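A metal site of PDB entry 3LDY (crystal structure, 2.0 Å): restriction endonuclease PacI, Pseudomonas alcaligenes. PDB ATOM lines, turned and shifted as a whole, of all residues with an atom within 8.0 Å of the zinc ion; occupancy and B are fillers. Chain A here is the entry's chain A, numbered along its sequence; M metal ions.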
ATOM      1  N   HIS A  62     -13.750 -16.080  20.381  1.00  0.00           N
ATOM      2  CA  HIS A  62     -15.079 -16.584  20.748  1.00  0.00           C
ATOM      3  C   HIS A  62     -15.965 -15.368  20.969  1.00  0.00           C
ATOM      4  O   HIS A  62     -15.504 -14.345  21.498  1.00  0.00           O
ATOM      5  CB  HIS A  62     -15.046 -17.383  22.059  1.00  0.00           C
ATOM      6  CG  HIS A  62     -14.126 -18.555  22.039  1.00  0.00           C
ATOM      7  ND1 HIS A  62     -14.581 -19.854  22.066  1.00  0.00           N
ATOM      8  CD2 HIS A  62     -12.769 -18.623  22.017  1.00  0.00           C
ATOM      9  CE1 HIS A  62     -13.545 -20.673  22.051  1.00  0.00           C
ATOM     10  NE2 HIS A  62     -12.440 -19.955  22.010  1.00  0.00           N
ATOM     11  N   CYS A  63     -17.224 -15.481  20.542  1.00  0.00           N
ATOM     12  CA  CYS A  63     -18.226 -14.474  20.764  1.00  0.00           C
ATOM     13  C   CYS A  63     -18.293 -14.126  22.264  1.00  0.00           C
ATOM     14  O   CYS A  63     -18.388 -15.030  23.090  1.00  0.00           O
ATOM     15  CB  CYS A  63     -19.578 -15.023  20.300  1.00  0.00           C
ATOM     16  SG  CYS A  63     -20.941 -13.852  20.539  1.00  0.00           S
ATOM     17  N   GLY A  64     -18.236 -12.840  22.617  1.00  0.00           N
ATOM     18  CA  GLY A  64     -18.269 -12.435  24.054  1.00  0.00           C
ATOM     19  C   GLY A  64     -19.672 -12.468  24.658  1.00  0.00           C
ATOM     20  O   GLY A  64     -19.856 -12.164  25.839  1.00  0.00           O
ATOM     21  N   TYR A  65     -20.678 -12.797  23.845  1.00  0.00           N
ATOM     22  CA  TYR A  65     -22.027 -13.081  24.350  1.00  0.00           C
ATOM     23  C   TYR A  65     -22.375 -14.576  24.505  1.00  0.00           C
ATOM     24  O   TYR A  65     -22.742 -15.018  25.609  1.00  0.00           O
ATOM     25  CB  TYR A  65     -23.064 -12.358  23.482  1.00  0.00           C
ATOM     26  CG  TYR A  65     -22.879 -10.868  23.582  1.00  0.00           C
ATOM     27  CD1 TYR A  65     -22.513 -10.112  22.460  1.00  0.00           C
ATOM     28  CD2 TYR A  65     -23.015 -10.207  24.820  1.00  0.00           C
ATOM     29  CE1 TYR A  65     -22.310  -8.724  22.585  1.00  0.00           C
ATOM     30  CE2 TYR A  65     -22.811  -8.837  24.936  1.00  0.00           C
ATOM     31  CZ  TYR A  65     -22.462  -8.109  23.823  1.00  0.00           C
ATOM     32  OH  TYR A  65     -22.288  -6.741  23.940  1.00  0.00           O
ATOM     33  N   CYS A  66     -22.267 -15.348  23.415  1.00  0.00           N
ATOM     34  CA  CYS A  66     -22.726 -16.749  23.423  1.00  0.00           C
ATOM     35  C   CYS A  66     -21.590 -17.762  23.618  1.00  0.00           C
ATOM     36  O   CYS A  66     -21.855 -18.939  23.864  1.00  0.00           O
ATOM     37  CB  CYS A  66     -23.563 -17.107  22.180  1.00  0.00           C
ATOM     38  SG  CYS A  66     -22.628 -17.280  20.600  1.00  0.00           S
ATOM     39  N   GLY A  67     -20.350 -17.303  23.503  1.00  0.00           N
ATOM     40  CA  GLY A  67     -19.175 -18.164  23.671  1.00  0.00           C
ATOM     41  C   GLY A  67     -18.814 -19.030  22.460  1.00  0.00           C
ATOM     42  O   GLY A  67     -17.841 -19.774  22.533  1.00  0.00           O
ATOM     43  N   ILE A  68     -19.556 -18.939  21.361  1.00  0.00           N
ATOM     44  CA  ILE A  68     -19.237 -19.772  20.192  1.00  0.00           C
ATOM     45  C   ILE A  68     -17.843 -19.427  19.637  1.00  0.00           C
ATOM     46  O   ILE A  68     -17.504 -18.251  19.509  1.00  0.00           O
ATOM     47  CB  ILE A  68     -20.313 -19.640  19.069  1.00  0.00           C
ATOM     48  CG1 ILE A  68     -20.282 -20.854  18.128  1.00  0.00           C
ATOM     49  CG2 ILE A  68     -20.152 -18.360  18.263  1.00  0.00           C
ATOM     50  CD1 ILE A  68     -21.491 -20.877  17.249  1.00  0.00           C
ATOM     51  N   SER A  69     -17.053 -20.460  19.314  1.00  0.00           N
ATOM     52  CA  SER A  69     -15.719 -20.280  18.724  1.00  0.00           C
ATOM     53  C   SER A  69     -15.936 -19.796  17.308  1.00  0.00           C
ATOM     54  O   SER A  69     -17.013 -20.002  16.732  1.00  0.00           O
ATOM     55  CB  SER A  69     -14.942 -21.595  18.684  1.00  0.00           C
ATOM     56  OG  SER A  69     -15.560 -22.520  17.777  1.00  0.00           O
ATOM     57  N   PHE A  73     -18.859 -20.957  14.650  1.00  0.00           N
ATOM     58  CA  PHE A  73     -19.735 -20.020  13.950  1.00  0.00           C
ATOM     59  C   PHE A  73     -19.699 -20.221  12.425  1.00  0.00           C
ATOM     60  O   PHE A  73     -20.716 -20.167  11.742  1.00  0.00           O
ATOM     61  CB  PHE A  73     -19.409 -18.573  14.300  1.00  0.00           C
ATOM     62  CG  PHE A  73     -20.468 -17.637  13.824  1.00  0.00           C
ATOM     63  CD1 PHE A  73     -21.724 -17.598  14.455  1.00  0.00           C
ATOM     64  CD2 PHE A  73     -20.263 -16.878  12.681  1.00  0.00           C
ATOM     65  CE1 PHE A  73     -22.696 -16.764  13.990  1.00  0.00           C
ATOM     66  CE2 PHE A  73     -21.266 -16.019  12.230  1.00  0.00           C
ATOM     67  CZ  PHE A  73     -22.471 -15.986  12.877  1.00  0.00           C
ATOM     68  N   LEU A  76     -21.948 -22.785  11.041  1.00  0.00           N
ATOM     69  CA  LEU A  76     -23.384 -22.515  10.924  1.00  0.00           C
ATOM     70  C   LEU A  76     -23.759 -22.042   9.513  1.00  0.00           C
ATOM     71  O   LEU A  76     -24.940 -21.927   9.199  1.00  0.00           O
ATOM     72  CB  LEU A  76     -23.822 -21.464  11.965  1.00  0.00           C
ATOM     73  CG  LEU A  76     -23.776 -21.754  13.468  1.00  0.00           C
ATOM     74  CD1 LEU A  76     -24.225 -20.533  14.203  1.00  0.00           C
ATOM     75  CD2 LEU A  76     -24.714 -22.895  13.754  1.00  0.00           C
ATOM     76  N   LEU A  89     -15.494 -13.737  13.432  1.00  0.00           N
ATOM     77  CA  LEU A  89     -16.304 -13.014  14.396  1.00  0.00           C
ATOM     78  C   LEU A  89     -16.037 -11.528  14.207  1.00  0.00           C
ATOM     79  O   LEU A  89     -14.941 -11.142  13.828  1.00  0.00           O
ATOM     80  CB  LEU A  89     -15.969 -13.468  15.830  1.00  0.00           C
ATOM     81  CG  LEU A  89     -16.183 -14.973  16.062  1.00  0.00           C
ATOM     82  CD1 LEU A  89     -15.827 -15.295  17.484  1.00  0.00           C
ATOM     83  CD2 LEU A  89     -17.625 -15.440  15.758  1.00  0.00           C
ATOM     84  N   LEU A 107     -15.855  -8.508  21.027  1.00  0.00           N
ATOM     85  CA  LEU A 107     -15.982  -9.507  19.982  1.00  0.00           C
ATOM     86  C   LEU A 107     -17.363 -10.123  20.037  1.00  0.00           C
ATOM     87  O   LEU A 107     -17.821 -10.570  21.120  1.00  0.00           O
ATOM     88  CB  LEU A 107     -14.941 -10.593  20.179  1.00  0.00           C
ATOM     89  CG  LEU A 107     -14.378 -11.216  18.910  1.00  0.00           C
ATOM     90  CD1 LEU A 107     -13.752 -10.195  17.975  1.00  0.00           C
ATOM     91  CD2 LEU A 107     -13.392 -12.312  19.274  1.00  0.00           C
ATOM     92  N   ALA A 108     -18.071 -10.105  18.910  1.00  0.00           N
ATOM     93  CA  ALA A 108     -19.359 -10.812  18.867  1.00  0.00           C
ATOM     94  C   ALA A 108     -19.624 -11.538  17.520  1.00  0.00           C
ATOM     95  O   ALA A 108     -19.208 -11.044  16.452  1.00  0.00           O
ATOM     96  CB  ALA A 108     -20.504  -9.861  19.204  1.00  0.00           C
ATOM     97  N   CYS A 109     -20.309 -12.673  17.579  1.00  0.00           N
ATOM     98  CA  CYS A 109     -20.722 -13.370  16.336  1.00  0.00           C
ATOM     99  C   CYS A 109     -21.812 -12.527  15.646  1.00  0.00           C
ATOM    100  O   CYS A 109     -22.502 -11.792  16.316  1.00  0.00           O
ATOM    101  CB  CYS A 109     -21.249 -14.820  16.627  1.00  0.00           C
ATOM    102  SG  CYS A 109     -22.732 -15.062  17.759  1.00  0.00           S
ATOM    103  N   PHE A 110     -21.985 -12.647  14.334  1.00  0.00           N
ATOM    104  CA  PHE A 110     -23.012 -11.849  13.628  1.00  0.00           C
ATOM    105  C   PHE A 110     -24.452 -12.147  14.087  1.00  0.00           C
ATOM    106  O   PHE A 110     -25.355 -11.304  13.937  1.00  0.00           O
ATOM    107  CB  PHE A 110     -22.894 -12.068  12.123  1.00  0.00           C
ATOM    108  CG  PHE A 110     -23.464 -10.965  11.285  1.00  0.00           C
ATOM    109  CD1 PHE A 110     -23.308  -9.660  11.675  1.00  0.00           C
ATOM    110  CD2 PHE A 110     -24.135 -11.240  10.073  1.00  0.00           C
ATOM    111  CE1 PHE A 110     -23.832  -8.609  10.920  1.00  0.00           C
ATOM    112  CE2 PHE A 110     -24.639 -10.210   9.273  1.00  0.00           C
ATOM    113  CZ  PHE A 110     -24.493  -8.883   9.708  1.00  0.00           C
ATOM    114  N   ILE A 111     -24.688 -13.335  14.618  1.00  0.00           N
ATOM    115  CA  ILE A 111     -26.013 -13.662  15.167  1.00  0.00           C
ATOM    116  C   ILE A 111     -26.280 -12.831  16.433  1.00  0.00           C
ATOM    117  O   ILE A 111     -27.295 -12.142  16.526  1.00  0.00           O
ATOM    118  CB  ILE A 111     -26.185 -15.192  15.406  1.00  0.00           C
ATOM    119  CG1 ILE A 111     -26.482 -15.879  14.070  1.00  0.00           C
ATOM    120  CG2 ILE A 111     -27.330 -15.459  16.402  1.00  0.00           C
ATOM    121  CD1 ILE A 111     -26.311 -17.406  14.075  1.00  0.00           C
ATOM    122  N   CYS A 112     -25.348 -12.827  17.388  1.00  0.00           N
ATOM    123  CA  CYS A 112     -25.561 -12.068  18.602  1.00  0.00           C
ATOM    124  C   CYS A 112     -25.569 -10.564  18.328  1.00  0.00           C
ATOM    125  O   CYS A 112     -26.301  -9.804  18.968  1.00  0.00           O
ATOM    126  CB  CYS A 112     -24.474 -12.404  19.620  1.00  0.00           C
ATOM    127  SG  CYS A 112     -24.816 -13.984  20.441  1.00  0.00           S
ATOM    128  N   ASN A 113     -24.712 -10.154  17.401  1.00  0.00           N
ATOM    129  CA  ASN A 113     -24.576  -8.734  17.064  1.00  0.00           C
ATOM    130  C   ASN A 113     -25.877  -8.117  16.508  1.00  0.00           C
ATOM    131  O   ASN A 113     -26.268  -7.023  16.903  1.00  0.00           O
ATOM    132  CB  ASN A 113     -23.405  -8.537  16.098  1.00  0.00           C
ATOM    133  CG  ASN A 113     -22.639  -7.262  16.387  1.00  0.00           C
ATOM    134  OD1 ASN A 113     -23.078  -6.450  17.193  1.00  0.00           O
ATOM    135  ND2 ASN A 113     -21.475  -7.092  15.780  1.00  0.00           N
ATOM    136  N   ILE A 115     -28.901  -9.644  16.945  1.00  0.00           N
ATOM    137  CA  ILE A 115     -29.924  -9.747  18.005  1.00  0.00           C
ATOM    138  C   ILE A 115     -29.905  -8.535  18.953  1.00  0.00           C
ATOM    139  O   ILE A 115     -30.942  -7.889  19.217  1.00  0.00           O
ATOM    140  CB  ILE A 115     -29.832 -11.087  18.753  1.00  0.00           C
ATOM    141  CG1 ILE A 115     -30.349 -12.207  17.817  1.00  0.00           C
ATOM    142  CG2 ILE A 115     -30.606 -11.034  20.103  1.00  0.00           C
ATOM    143  CD1 ILE A 115     -29.927 -13.542  18.219  1.00  0.00           C
ATOM    144  N   MET A 125     -27.624  -8.145  27.056  1.00  0.00           N
ATOM    145  CA  MET A 125     -27.191  -9.099  26.043  1.00  0.00           C
ATOM    146  C   MET A 125     -26.353 -10.271  26.648  1.00  0.00           C
ATOM    147  O   MET A 125     -26.384 -11.405  26.135  1.00  0.00           O
ATOM    148  CB  MET A 125     -26.470  -8.409  24.886  1.00  0.00           C
ATOM    149  CG  MET A 125     -26.303  -9.373  23.694  1.00  0.00           C
ATOM    150  SD  MET A 125     -27.878  -9.870  22.933  1.00  0.00           S
ATOM    151  CE  MET A 125     -27.406 -11.373  22.029  1.00  0.00           C
ATOM    152  N   LEU A 128     -29.015 -12.741  27.354  1.00  0.00           N
ATOM    153  CA  LEU A 128     -29.445 -13.362  26.072  1.00  0.00           C
ATOM    154  C   LEU A 128     -28.381 -14.361  25.580  1.00  0.00           C
ATOM    155  O   LEU A 128     -28.693 -15.470  25.121  1.00  0.00           O
ATOM    156  CB  LEU A 128     -29.708 -12.325  24.978  1.00  0.00           C
ATOM    157  CG  LEU A 128     -31.148 -11.879  24.760  1.00  0.00           C
ATOM    158  CD1 LEU A 128     -31.383 -11.000  23.560  1.00  0.00           C
ATOM    159  CD2 LEU A 128     -31.836 -13.122  24.481  1.00  0.00           C
ATOM    160  N   GLY A 129     -27.113 -13.943  25.678  1.00  0.00           N
ATOM    161  CA  GLY A 129     -26.001 -14.751  25.214  1.00  0.00           C
ATOM    162  C   GLY A 129     -25.979 -16.161  25.806  1.00  0.00           C
ATOM    163  O   GLY A 129     -25.746 -17.140  25.086  1.00  0.00           O
ATOM    164  N   ILE A 132     -28.636 -18.200  24.065  1.00  0.00           N
ATOM    165  CA  ILE A 132     -28.100 -18.569  22.760  1.00  0.00           C
ATOM    166  C   ILE A 132     -27.078 -19.731  22.840  1.00  0.00           C
ATOM    167  O   ILE A 132     -27.162 -20.663  22.040  1.00  0.00           O
ATOM    168  CB  ILE A 132     -27.524 -17.324  22.021  1.00  0.00           C
ATOM    169  CG1 ILE A 132     -28.669 -16.356  21.737  1.00  0.00           C
ATOM    170  CG2 ILE A 132     -26.915 -17.747  20.717  1.00  0.00           C
ATOM    171  CD1 ILE A 132     -28.240 -14.892  21.256  1.00  0.00           C
ATOM    172  N   SER A 133     -26.189 -19.685  23.819  1.00  0.00           N
ATOM    173  CA  SER A 133     -25.218 -20.763  24.058  1.00  0.00           C
ATOM    174  C   SER A 133     -25.883 -22.127  24.279  1.00  0.00           C
ATOM    175  O   SER A 133     -25.356 -23.154  23.875  1.00  0.00           O
ATOM    176  CB  SER A 133     -24.359 -20.444  25.269  1.00  0.00           C
ATOM    177  OG  SER A 133     -23.276 -21.342  25.301  1.00  0.00           O
ATOM    178  N   TRP A 136     -26.747 -23.529  20.890  1.00  0.00           N
ATOM    179  CA  TRP A 136     -25.544 -24.110  20.300  1.00  0.00           C
ATOM    180  C   TRP A 136     -25.166 -25.417  20.990  1.00  0.00           C
ATOM    181  O   TRP A 136     -24.939 -26.433  20.318  1.00  0.00           O
ATOM    182  CB  TRP A 136     -24.375 -23.120  20.350  1.00  0.00           C
ATOM    183  CG  TRP A 136     -24.578 -21.695  19.732  1.00  0.00           C
ATOM    184  CD1 TRP A 136     -23.931 -20.542  20.113  1.00  0.00           C
ATOM    185  CD2 TRP A 136     -25.460 -21.309  18.636  1.00  0.00           C
ATOM    186  NE1 TRP A 136     -24.326 -19.482  19.332  1.00  0.00           N
ATOM    187  CE2 TRP A 136     -25.278 -19.914  18.440  1.00  0.00           C
ATOM    188  CE3 TRP A 136     -26.392 -22.000  17.835  1.00  0.00           C
ATOM    189  CZ2 TRP A 136     -25.987 -19.194  17.459  1.00  0.00           C
ATOM    190  CZ3 TRP A 136     -27.080 -21.302  16.853  1.00  0.00           C
ATOM    191  CH2 TRP A 136     -26.897 -19.899  16.684  1.00  0.00           C
HETATM  192 ZN    ZN M   1     -22.798 -15.097  19.761  1.00  0.00          ZN
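The backbone NH of Ile 68 lies close to the side-chain sulfur of Cys 66 (3.6 Å).
The side-chain sulfur (SG) of Cys 66 lies close to the indole nitrogen (NE1) of Trp 136.
OG of Ser 133 sits at hydrogen-bond distance from O of Cys 66, 3.1 Å away.
The backbone NH of Cys 63 lies within hydrogen-bond range of the backbone carbonyl oxygen of Ile 68 (3.0 Å).
The side-chain sulfur (SG) of Cys 63 sits close to the backbone NH (N) of Tyr 65.
The zinc ion is bound by SG of Cys 109 (2.0 Å).
The zinc ion is bound by SG of Cys 66.
The zinc ion is bound by the side-chain sulfur (SG) of Cys 63, 2.4 Å away.
SG of Cys 112 is bound to the zinc ion (2.4 Å).
The zinc ion has four donor atoms within binding distance.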
